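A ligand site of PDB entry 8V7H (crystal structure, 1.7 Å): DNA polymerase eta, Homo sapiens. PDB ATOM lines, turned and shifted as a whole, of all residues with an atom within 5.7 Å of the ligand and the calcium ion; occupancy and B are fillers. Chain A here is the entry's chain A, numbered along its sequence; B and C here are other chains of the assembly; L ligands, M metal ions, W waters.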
ATOM      1  N   ASP A  16     -19.113   5.459  17.620  1.00  0.00           N
ATOM      2  CA  ASP A  16     -20.034   4.833  18.598  1.00  0.00           C
ATOM      3  C   ASP A  16     -19.409   3.549  19.142  1.00  0.00           C
ATOM      4  O   ASP A  16     -19.307   2.572  18.366  1.00  0.00           O
ATOM      5  CB  ASP A  16     -21.340   4.561  17.842  1.00  0.00           C
ATOM      6  CG  ASP A  16     -22.549   4.256  18.706  1.00  0.00           C
ATOM      7  OD1 ASP A  16     -22.406   3.423  19.605  1.00  0.00           O
ATOM      8  OD2 ASP A  16     -23.622   4.826  18.446  1.00  0.00           O
ATOM      9  N   MET A  17     -19.006   3.533  20.419  1.00  0.00           N
ATOM     10  CA  MET A  17     -18.361   2.337  21.006  1.00  0.00           C
ATOM     11  C   MET A  17     -19.380   1.190  20.983  1.00  0.00           C
ATOM     12  O   MET A  17     -20.433   1.339  21.567  1.00  0.00           O
ATOM     13  CB  MET A  17     -17.886   2.621  22.431  1.00  0.00           C
ATOM     14  CG  MET A  17     -16.992   3.835  22.534  1.00  0.00           C
ATOM     15  SD  MET A  17     -15.618   3.754  21.363  1.00  0.00           S
ATOM     16  CE  MET A  17     -14.910   2.162  21.798  1.00  0.00           C
ATOM     17  N   ASP A  18     -19.029   0.101  20.312  1.00  0.00           N
ATOM     18  CA  ASP A  18     -19.916  -1.084  20.224  1.00  0.00           C
ATOM     19  C   ASP A  18     -20.234  -1.603  21.626  1.00  0.00           C
ATOM     20  O   ASP A  18     -19.310  -1.726  22.413  1.00  0.00           O
ATOM     21  CB  ASP A  18     -19.299  -2.162  19.335  1.00  0.00           C
ATOM     22  CG  ASP A  18     -19.097  -1.735  17.890  1.00  0.00           C
ATOM     23  OD1 ASP A  18     -19.909  -0.941  17.392  1.00  0.00           O
ATOM     24  OD2 ASP A  18     -18.135  -2.217  17.276  1.00  0.00           O
ATOM     25  N   CYS A  19     -21.506  -1.884  21.923  1.00  0.00           N
ATOM     26  CA  CYS A  19     -21.979  -2.386  23.223  1.00  0.00           C
ATOM     27  C   CYS A  19     -21.027  -2.048  24.363  1.00  0.00           C
ATOM     28  O   CYS A  19     -20.405  -2.948  24.951  1.00  0.00           O
ATOM     29  CB  CYS A  19     -22.208  -3.899  23.169  1.00  0.00           C
ATOM     30  SG  CYS A  19     -20.911  -4.898  22.442  1.00  0.00           S
ATOM     31  N   PHE A  20     -20.933  -0.751  24.697  1.00  0.00           N
ATOM     32  CA  PHE A  20     -19.771  -0.234  25.411  1.00  0.00           C
ATOM     33  C   PHE A  20     -19.587  -0.873  26.789  1.00  0.00           C
ATOM     34  O   PHE A  20     -18.488  -1.341  27.116  1.00  0.00           O
ATOM     35  CB  PHE A  20     -19.853   1.271  25.563  1.00  0.00           C
ATOM     36  CG  PHE A  20     -18.625   1.856  26.187  1.00  0.00           C
ATOM     37  CD1 PHE A  20     -17.361   1.475  25.731  1.00  0.00           C
ATOM     38  CD2 PHE A  20     -18.718   2.735  27.266  1.00  0.00           C
ATOM     39  CE1 PHE A  20     -16.203   1.973  26.306  1.00  0.00           C
ATOM     40  CE2 PHE A  20     -17.555   3.247  27.864  1.00  0.00           C
ATOM     41  CZ  PHE A  20     -16.308   2.865  27.371  1.00  0.00           C
ATOM     42  N   PHE A  21     -20.626  -0.862  27.633  1.00  0.00           N
ATOM     43  CA  PHE A  21     -20.452  -1.394  28.982  1.00  0.00           C
ATOM     44  C   PHE A  21     -20.024  -2.863  28.924  1.00  0.00           C
ATOM     45  O   PHE A  21     -19.219  -3.316  29.746  1.00  0.00           O
ATOM     46  CB  PHE A  21     -21.743  -1.267  29.794  1.00  0.00           C
ATOM     47  CG  PHE A  21     -22.100   0.133  30.208  1.00  0.00           C
ATOM     48  CD1 PHE A  21     -21.535   1.254  29.598  1.00  0.00           C
ATOM     49  CD2 PHE A  21     -23.023   0.333  31.238  1.00  0.00           C
ATOM     50  CE1 PHE A  21     -21.905   2.538  30.001  1.00  0.00           C
ATOM     51  CE2 PHE A  21     -23.374   1.606  31.636  1.00  0.00           C
ATOM     52  CZ  PHE A  21     -22.810   2.705  31.013  1.00  0.00           C
ATOM     53  N   VAL A  22     -20.559  -3.606  27.945  1.00  0.00           N
ATOM     54  CA  VAL A  22     -20.144  -5.002  27.718  1.00  0.00           C
ATOM     55  C   VAL A  22     -18.657  -5.078  27.406  1.00  0.00           C
ATOM     56  O   VAL A  22     -17.933  -5.914  27.957  1.00  0.00           O
ATOM     57  CB  VAL A  22     -20.986  -5.633  26.606  1.00  0.00           C
ATOM     58  CG1 VAL A  22     -20.371  -6.970  26.163  1.00  0.00           C
ATOM     59  CG2 VAL A  22     -22.410  -5.851  27.067  1.00  0.00           C
ATOM     60  N   GLN A  41     -28.033  -4.164  35.797  1.00  0.00           N
ATOM     61  CA  GLN A  41     -28.086  -3.339  37.001  1.00  0.00           C
ATOM     62  C   GLN A  41     -29.032  -4.011  37.979  1.00  0.00           C
ATOM     63  O   GLN A  41     -30.168  -4.353  37.600  1.00  0.00           O
ATOM     64  CB  GLN A  41     -28.602  -1.918  36.754  1.00  0.00           C
ATOM     65  CG  GLN A  41     -27.725  -1.058  35.913  1.00  0.00           C
ATOM     66  CD  GLN A  41     -28.216   0.371  35.791  1.00  0.00           C
ATOM     67  OE1 GLN A  41     -27.416   1.308  35.899  1.00  0.00           O
ATOM     68  NE2 GLN A  41     -29.521   0.538  35.568  1.00  0.00           N
ATOM     69  N   ILE A  51     -28.789  -3.603  30.585  1.00  0.00           N
ATOM     70  CA  ILE A  51     -28.537  -2.295  29.991  1.00  0.00           C
ATOM     71  C   ILE A  51     -27.559  -2.357  28.830  1.00  0.00           C
ATOM     72  O   ILE A  51     -27.433  -1.341  28.113  1.00  0.00           O
ATOM     73  CB  ILE A  51     -28.046  -1.266  31.015  1.00  0.00           C
ATOM     74  CG1 ILE A  51     -26.792  -1.750  31.738  1.00  0.00           C
ATOM     75  CG2 ILE A  51     -29.163  -0.963  32.051  1.00  0.00           C
ATOM     76  CD1 ILE A  51     -26.367  -0.846  32.828  1.00  0.00           C
ATOM     77  N   ALA A  52     -26.848  -3.464  28.622  1.00  0.00           N
ATOM     78  CA  ALA A  52     -26.013  -3.573  27.412  1.00  0.00           C
ATOM     79  C   ALA A  52     -25.868  -5.036  27.008  1.00  0.00           C
ATOM     80  O   ALA A  52     -25.905  -5.914  27.857  1.00  0.00           O
ATOM     81  CB  ALA A  52     -24.605  -2.948  27.591  1.00  0.00           C
ATOM     82  N   VAL A  53     -25.715  -5.289  25.694  1.00  0.00           N
ATOM     83  CA  VAL A  53     -25.815  -6.633  25.146  1.00  0.00           C
ATOM     84  C   VAL A  53     -24.770  -6.830  24.061  1.00  0.00           C
ATOM     85  O   VAL A  53     -24.724  -6.041  23.104  1.00  0.00           O
ATOM     86  CB  VAL A  53     -27.214  -6.884  24.550  1.00  0.00           C
ATOM     87  CG1 VAL A  53     -27.371  -8.324  24.209  1.00  0.00           C
ATOM     88  CG2 VAL A  53     -28.323  -6.407  25.495  1.00  0.00           C
ATOM     89  N   TYR A  55     -22.987  -8.548  20.761  1.00  0.00           N
ATOM     90  CA  TYR A  55     -23.662  -8.890  19.510  1.00  0.00           C
ATOM     91  C   TYR A  55     -23.987 -10.386  19.426  1.00  0.00           C
ATOM     92  O   TYR A  55     -25.036 -10.763  18.863  1.00  0.00           O
ATOM     93  CB  TYR A  55     -22.819  -8.412  18.328  1.00  0.00           C
ATOM     94  CG  TYR A  55     -23.004  -6.920  18.098  1.00  0.00           C
ATOM     95  CD1 TYR A  55     -22.355  -5.980  18.905  1.00  0.00           C
ATOM     96  CD2 TYR A  55     -23.871  -6.451  17.120  1.00  0.00           C
ATOM     97  CE1 TYR A  55     -22.546  -4.611  18.718  1.00  0.00           C
ATOM     98  CE2 TYR A  55     -24.066  -5.089  16.921  1.00  0.00           C
ATOM     99  CZ  TYR A  55     -23.408  -4.162  17.709  1.00  0.00           C
ATOM    100  OH  TYR A  55     -23.624  -2.816  17.492  1.00  0.00           O
ATOM    101  N   ARG A  58     -27.244 -10.537  21.204  1.00  0.00           N
ATOM    102  CA  ARG A  58     -28.310  -9.940  20.370  1.00  0.00           C
ATOM    103  C   ARG A  58     -28.848 -10.925  19.354  1.00  0.00           C
ATOM    104  O   ARG A  58     -30.041 -10.883  19.023  1.00  0.00           O
ATOM    105  CB  ARG A  58     -27.784  -8.694  19.650  1.00  0.00           C
ATOM    106  CG  ARG A  58     -27.442  -7.569  20.589  1.00  0.00           C
ATOM    107  CD  ARG A  58     -26.926  -6.380  19.831  1.00  0.00           C
ATOM    108  NE  ARG A  58     -26.273  -5.427  20.713  1.00  0.00           N
ATOM    109  CZ  ARG A  58     -26.024  -4.161  20.389  1.00  0.00           C
ATOM    110  NH1 ARG A  58     -26.314  -3.690  19.187  1.00  0.00           N
ATOM    111  NH2 ARG A  58     -25.471  -3.357  21.293  1.00  0.00           N
ATOM    112  N   ARG A  64     -31.582  -4.494  25.369  1.00  0.00           N
ATOM    113  CA  ARG A  64     -31.594  -3.599  26.538  1.00  0.00           C
ATOM    114  C   ARG A  64     -33.040  -3.421  27.007  1.00  0.00           C
ATOM    115  O   ARG A  64     -34.007  -3.612  26.260  1.00  0.00           O
ATOM    116  CB  ARG A  64     -30.990  -2.249  26.176  1.00  0.00           C
ATOM    117  CG  ARG A  64     -30.913  -1.249  27.328  1.00  0.00           C
ATOM    118  CD  ARG A  64     -30.013  -0.069  27.019  1.00  0.00           C
ATOM    119  NE  ARG A  64     -29.826   0.170  25.599  1.00  0.00           N
ATOM    120  CZ  ARG A  64     -28.640   0.175  24.984  1.00  0.00           C
ATOM    121  NH1 ARG A  64     -27.532  -0.050  25.666  1.00  0.00           N
ATOM    122  NH2 ARG A  64     -28.573   0.402  23.682  1.00  0.00           N
ATOM    123  N   SER A 116     -22.525  11.339  24.234  1.00  0.00           N
ATOM    124  CA  SER A 116     -22.946  10.427  25.325  1.00  0.00           C
ATOM    125  C   SER A 116     -21.675   9.757  25.863  1.00  0.00           C
ATOM    126  O   SER A 116     -20.604  10.016  25.321  1.00  0.00           O
ATOM    127  CB  SER A 116     -23.936   9.393  24.855  1.00  0.00           C
ATOM    128  OG  SER A 116     -23.270   8.302  24.233  1.00  0.00           O
ATOM    129  N   ILE A 117     -21.815   8.898  26.859  1.00  0.00           N
ATOM    130  CA  ILE A 117     -20.648   8.170  27.413  1.00  0.00           C
ATOM    131  C   ILE A 117     -19.961   7.326  26.340  1.00  0.00           C
ATOM    132  O   ILE A 117     -18.775   7.080  26.477  1.00  0.00           O
ATOM    133  CB  ILE A 117     -21.095   7.268  28.581  1.00  0.00           C
ATOM    134  CG1 ILE A 117     -19.929   6.805  29.446  1.00  0.00           C
ATOM    135  CG2 ILE A 117     -21.923   6.098  28.081  1.00  0.00           C
ATOM    136  CD1 ILE A 117     -20.349   6.231  30.769  1.00  0.00           C
ATOM    137  N   ASP A 118     -20.680   6.946  25.283  1.00  0.00           N
ATOM    138  CA  ASP A 118     -20.123   6.005  24.299  1.00  0.00           C
ATOM    139  C   ASP A 118     -20.213   6.528  22.859  1.00  0.00           C
ATOM    140  O   ASP A 118     -20.032   5.743  21.932  1.00  0.00           O
ATOM    141  CB  ASP A 118     -20.927   4.720  24.379  1.00  0.00           C
ATOM    142  CG  ASP A 118     -21.850   4.615  23.199  1.00  0.00           C
ATOM    143  OD1 ASP A 118     -22.886   5.313  23.233  1.00  0.00           O
ATOM    144  OD2 ASP A 118     -21.477   3.884  22.263  1.00  0.00           O
ATOM    145  N   GLU A 119     -20.448   7.820  22.696  1.00  0.00           N
ATOM    146  CA  GLU A 119     -20.660   8.390  21.357  1.00  0.00           C
ATOM    147  C   GLU A 119     -20.059   9.783  21.281  1.00  0.00           C
ATOM    148  O   GLU A 119     -20.312  10.573  22.197  1.00  0.00           O
ATOM    149  CB  GLU A 119     -22.152   8.541  21.093  1.00  0.00           C
ATOM    150  CG  GLU A 119     -22.769   7.383  20.336  1.00  0.00           C
ATOM    151  CD  GLU A 119     -24.206   7.658  19.951  1.00  0.00           C
ATOM    152  OE1 GLU A 119     -24.566   8.834  19.803  1.00  0.00           O
ATOM    153  OE2 GLU A 119     -24.952   6.693  19.806  1.00  0.00           O
ATOM    154  N   LYS A 234     -22.773  -2.408  11.633  1.00  0.00           N
ATOM    155  CA  LYS A 234     -22.207  -2.624  12.971  1.00  0.00           C
ATOM    156  C   LYS A 234     -22.140  -4.146  13.161  1.00  0.00           C
ATOM    157  O   LYS A 234     -22.910  -4.862  12.498  1.00  0.00           O
ATOM    158  CB  LYS A 234     -23.080  -1.911  13.997  1.00  0.00           C
ATOM    159  CG  LYS A 234     -22.944  -0.404  14.083  1.00  0.00           C
ATOM    160  CD  LYS A 234     -23.621   0.181  15.312  1.00  0.00           C
ATOM    161  CE  LYS A 234     -22.942   1.423  15.852  1.00  0.00           C
ATOM    162  NZ  LYS A 234     -21.993   1.112  16.951  1.00  0.00           N
ATOM    163  P   CAR B   8     -28.847   8.398  20.136  1.00  0.00           P
ATOM    164  OP1 CAR B   8     -28.505   9.588  19.290  1.00  0.00           O
ATOM    165  OP2 CAR B   8     -28.119   7.147  19.725  1.00  0.00           O
ATOM    166  O5' CAR B   8     -28.510   8.675  21.705  1.00  0.00           O
ATOM    167  C5' CAR B   8     -27.196   8.391  22.082  1.00  0.00           C
ATOM    168  C4' CAR B   8     -27.204   7.713  23.469  1.00  0.00           C
ATOM    169  O4' CAR B   8     -28.519   7.729  24.033  1.00  0.00           O
ATOM    170  C3' CAR B   8     -26.917   6.213  23.352  1.00  0.00           C
ATOM    171  O3' CAR B   8     -25.515   6.081  23.472  1.00  0.00           O
ATOM    172  C2' CAR B   8     -27.681   5.596  24.550  1.00  0.00           C
ATOM    173  O2' CAR B   8     -28.625   4.587  24.181  1.00  0.00           O
ATOM    174  C1' CAR B   8     -28.387   6.832  25.126  1.00  0.00           C
ATOM    175  N1  CAR B   8     -29.706   6.619  25.654  1.00  0.00           N
ATOM    176  C2  CAR B   8     -29.837   6.689  27.016  1.00  0.00           C
ATOM    177  O2  CAR B   8     -28.839   6.907  27.680  1.00  0.00           O
ATOM    178  N3  CAR B   8     -31.039   6.540  27.597  1.00  0.00           N
ATOM    179  C4  CAR B   8     -32.122   6.320  26.852  1.00  0.00           C
ATOM    180  N4  CAR B   8     -33.293   6.168  27.453  1.00  0.00           N
ATOM    181  C5  CAR B   8     -32.004   6.235  25.443  1.00  0.00           C
ATOM    182  C6  CAR B   8     -30.804   6.398  24.863  1.00  0.00           C
ATOM    183  P    DT C   4     -37.285   1.408  35.802  1.00  0.00           P
ATOM    184  OP1  DT C   4     -37.649   1.223  37.262  1.00  0.00           O
ATOM    185  OP2  DT C   4     -37.768   2.697  35.189  1.00  0.00           O
ATOM    186  O5'  DT C   4     -35.678   1.450  35.736  1.00  0.00           O
ATOM    187  C5'  DT C   4     -34.920   0.507  36.522  1.00  0.00           C
ATOM    188  C4'  DT C   4     -33.521   1.037  36.693  1.00  0.00           C
ATOM    189  O4'  DT C   4     -32.891   1.253  35.416  1.00  0.00           O
ATOM    190  C3'  DT C   4     -33.427   2.376  37.398  1.00  0.00           C
ATOM    191  O3'  DT C   4     -32.094   2.471  37.867  1.00  0.00           O
ATOM    192  C2'  DT C   4     -33.504   3.353  36.244  1.00  0.00           C
ATOM    193  C1'  DT C   4     -32.616   2.634  35.244  1.00  0.00           C
ATOM    194  N1   DT C   4     -32.952   2.938  33.859  1.00  0.00           N
ATOM    195  C2   DT C   4     -31.941   2.897  32.931  1.00  0.00           C
ATOM    196  O2   DT C   4     -30.787   2.630  33.214  1.00  0.00           O
ATOM    197  N3   DT C   4     -32.346   3.155  31.657  1.00  0.00           N
ATOM    198  C4   DT C   4     -33.611   3.446  31.223  1.00  0.00           C
ATOM    199  O4   DT C   4     -33.799   3.674  30.029  1.00  0.00           O
ATOM    200  C5   DT C   4     -34.624   3.485  32.245  1.00  0.00           C
ATOM    201  C7   DT C   4     -36.042   3.798  31.858  1.00  0.00           C
ATOM    202  C6   DT C   4     -34.251   3.216  33.508  1.00  0.00           C
ATOM    203  P    DG C   5     -31.704   3.674  38.817  1.00  0.00           P
ATOM    204  OP1  DG C   5     -31.139   3.060  40.035  1.00  0.00           O
ATOM    205  OP2  DG C   5     -32.866   4.623  38.952  1.00  0.00           O
ATOM    206  O5'  DG C   5     -30.606   4.434  37.978  1.00  0.00           O
ATOM    207  C5'  DG C   5     -29.393   3.780  37.667  1.00  0.00           C
ATOM    208  C4'  DG C   5     -28.584   4.668  36.773  1.00  0.00           C
ATOM    209  O4'  DG C   5     -29.238   4.772  35.473  1.00  0.00           O
ATOM    210  C3'  DG C   5     -28.443   6.096  37.277  1.00  0.00           C
ATOM    211  O3'  DG C   5     -27.155   6.557  36.976  1.00  0.00           O
ATOM    212  C2'  DG C   5     -29.484   6.845  36.471  1.00  0.00           C
ATOM    213  C1'  DG C   5     -29.356   6.118  35.140  1.00  0.00           C
ATOM    214  N9   DG C   5     -30.487   6.308  34.248  1.00  0.00           N
ATOM    215  C8   DG C   5     -31.802   6.542  34.595  1.00  0.00           C
ATOM    216  N7   DG C   5     -32.581   6.695  33.562  1.00  0.00           N
ATOM    217  C5   DG C   5     -31.719   6.560  32.464  1.00  0.00           C
ATOM    218  C6   DG C   5     -31.983   6.646  31.078  1.00  0.00           C
ATOM    219  O6   DG C   5     -33.061   6.843  30.499  1.00  0.00           O
ATOM    220  N1   DG C   5     -30.811   6.458  30.330  1.00  0.00           N
ATOM    221  C2   DG C   5     -29.561   6.227  30.857  1.00  0.00           C
ATOM    222  N2   DG C   5     -28.554   6.071  29.984  1.00  0.00           N
ATOM    223  N3   DG C   5     -29.312   6.156  32.145  1.00  0.00           N
ATOM    224  C4   DG C   5     -30.436   6.335  32.887  1.00  0.00           C
HETATM  225  P1  LIG L   1     -24.248  -0.606  20.187  1.00  0.00           P
HETATM  226  O1  LIG L   1     -25.514  -0.922  19.441  1.00  0.00           O
HETATM  227  O2  LIG L   1     -23.937   0.858  20.032  1.00  0.00           O
HETATM  228  O3  LIG L   1     -23.113  -1.422  19.630  1.00  0.00           O
HETATM  229  P2  LIG L   1     -24.376  -0.025  23.110  1.00  0.00           P
HETATM  230  O4  LIG L   1     -23.082   0.758  23.168  1.00  0.00           O
HETATM  231  O5  LIG L   1     -24.492  -0.843  24.379  1.00  0.00           O
HETATM  232  O6  LIG L   1     -24.425  -0.968  21.782  1.00  0.00           O
HETATM  233  P3  LIG L   1     -25.801   2.597  23.160  1.00  0.00           P
HETATM  234  O7  LIG L   1     -24.812   3.203  22.213  1.00  0.00           O
HETATM  235  O8  LIG L   1     -27.207   2.990  22.771  1.00  0.00           O
HETATM  236  O9  LIG L   1     -25.665   0.984  23.019  1.00  0.00           O
HETATM  237  O10 LIG L   1     -25.416   3.038  24.703  1.00  0.00           O
HETATM  238  C1  LIG L   1     -24.078   2.956  25.110  1.00  0.00           C
HETATM  239  C2  LIG L   1     -23.907   2.515  26.549  1.00  0.00           C
HETATM  240  O11 LIG L   1     -24.770   3.304  27.425  1.00  0.00           O
HETATM  241  C3  LIG L   1     -24.307   1.039  26.706  1.00  0.00           C
HETATM  242  O12 LIG L   1     -23.148   0.226  26.841  1.00  0.00           O
HETATM  243  C4  LIG L   1     -25.139   1.004  28.003  1.00  0.00           C
HETATM  244  C5  LIG L   1     -25.606   2.457  28.206  1.00  0.00           C
HETATM  245  N1  LIG L   1     -27.001   2.717  27.813  1.00  0.00           N
HETATM  246  C6  LIG L   1     -27.697   2.947  26.706  1.00  0.00           C
HETATM  247  N2  LIG L   1     -28.979   3.106  27.048  1.00  0.00           N
HETATM  248  C7  LIG L   1     -29.093   2.993  28.384  1.00  0.00           C
HETATM  249  C8  LIG L   1     -30.149   3.057  29.257  1.00  0.00           C
HETATM  250  N3  LIG L   1     -31.398   3.308  28.836  1.00  0.00           N
HETATM  251  N4  LIG L   1     -29.924   2.890  30.541  1.00  0.00           N
HETATM  252  C9  LIG L   1     -28.666   2.648  30.954  1.00  0.00           C
HETATM  253  N5  LIG L   1     -27.618   2.559  30.183  1.00  0.00           N
HETATM  254  C10 LIG L   1     -27.811   2.738  28.868  1.00  0.00           C
HETATM  255 CA    CA M   1     -22.713   2.157  21.301  1.00  0.00          CA
HETATM  256  O   HOH W   1     -30.779   3.079  24.051  1.00  0.00           O
HETATM  257  O   HOH W   2     -25.985  -2.869  24.147  1.00  0.00           O
HETATM  258  O   HOH W   3     -27.904  -1.043  20.449  1.00  0.00           O
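N3 of CAR 8 of chain B is in hydrogen-bond range of a nitrogen (N3) of the ligand (3.5 Å).
An oxygen (O8) of the ligand lies close to O2' of CAR 8 of chain B (2.6 Å).
The guanidinium group (NH1) of Arg 58 lies within salt-bridge range of an oxygen (O1) of the ligand, at 2.9 Å.
The guanidinium group of Arg 64 lies within salt-bridge range of an oxygen (O8) of the ligand (3.1 Å).
A nitrogen (N3) of the ligand lies within hydrogen-bond range of O4 of DT 4 of chain C, 2.7 Å away.
The side-chain amino group of Lys 234 is in salt-bridge range of an oxygen (O3) of the ligand.
N of Cys 19 is in hydrogen-bond range of O3 of the ligand (2.8 Å).
An oxygen (O12) of the ligand lies within hydrogen-bond range of the backbone NH (N) of Phe 21 (2.9 Å).
O12 of the ligand is in hydrogen-bond range of N of Phe 20 (3.2 Å).
The side-chain hydroxyl (OH) of Tyr 55 sits at hydrogen-bond distance from an oxygen (O3) of the ligand (2.6 Å).
The guanidinium group (NH1) of Arg 64 sits at hydrogen-bond distance from the backbone carbonyl oxygen (O) of Ile 51, at 2.8 Å.
O of Val 53 sits at hydrogen-bond distance from NE of Arg 58 (2.9 Å).
N of Asp 118 lies close to OG of Ser 116 (3.1 Å).
O3' of CAR 8 of chain B sits close to the side-chain carboxylate (OD1) of Asp 118.
The backbone carbonyl oxygen (O) of Asp 16 is in hydrogen-bond range of the side-chain amino group (NZ) of Lys 234 (3.4 Å).
OD2 of Asp 16 sits close to OE2 of Glu 119.
O3' of CAR 8 of chain B sits at hydrogen-bond distance from the side-chain hydroxyl (OG) of Ser 116 (3.2 Å).
The side-chain carboxylate of Asp 18 lies within salt-bridge range of the side-chain amino group of Lys 234, 3.0 Å away.
Asp 18 touches the ligand (CA to O3, 3.3 Å).
Ile 51 touches the ligand.
Ala 52 touches the ligand (CB to O12, 3.6 Å).
DG 5 of chain C touches the ligand.
Three residues have an atom within 4 Å of the calcium ion: Asp 16, Met 17 and Asp 118.
Along chain A the residues within 4 Å of the calcium ion span positions 16 to 118.
The calcium ion is bound by OD1 of Asp 16, O2 of the ligand, OD2 of Asp 118, O4 of the ligand, O of Met 17 and O7 of the ligand.
The calcium ion has six donor atoms within binding distance.
Water W2 lies within hydrogen-bond range of O5 of the ligand, N of Val 53 and NH2 of Arg 58.
Water W3 bridges an oxygen (O1) of the ligand and the guanidinium group (NH1) of Arg 58.
Water W1 lies within hydrogen-bond range of O2' of CAR 8 of chain B (2.6 Å), the guanidinium group of Arg 64 (3.4 Å) and a nitrogen (N2) of the ligand (3.5 Å).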
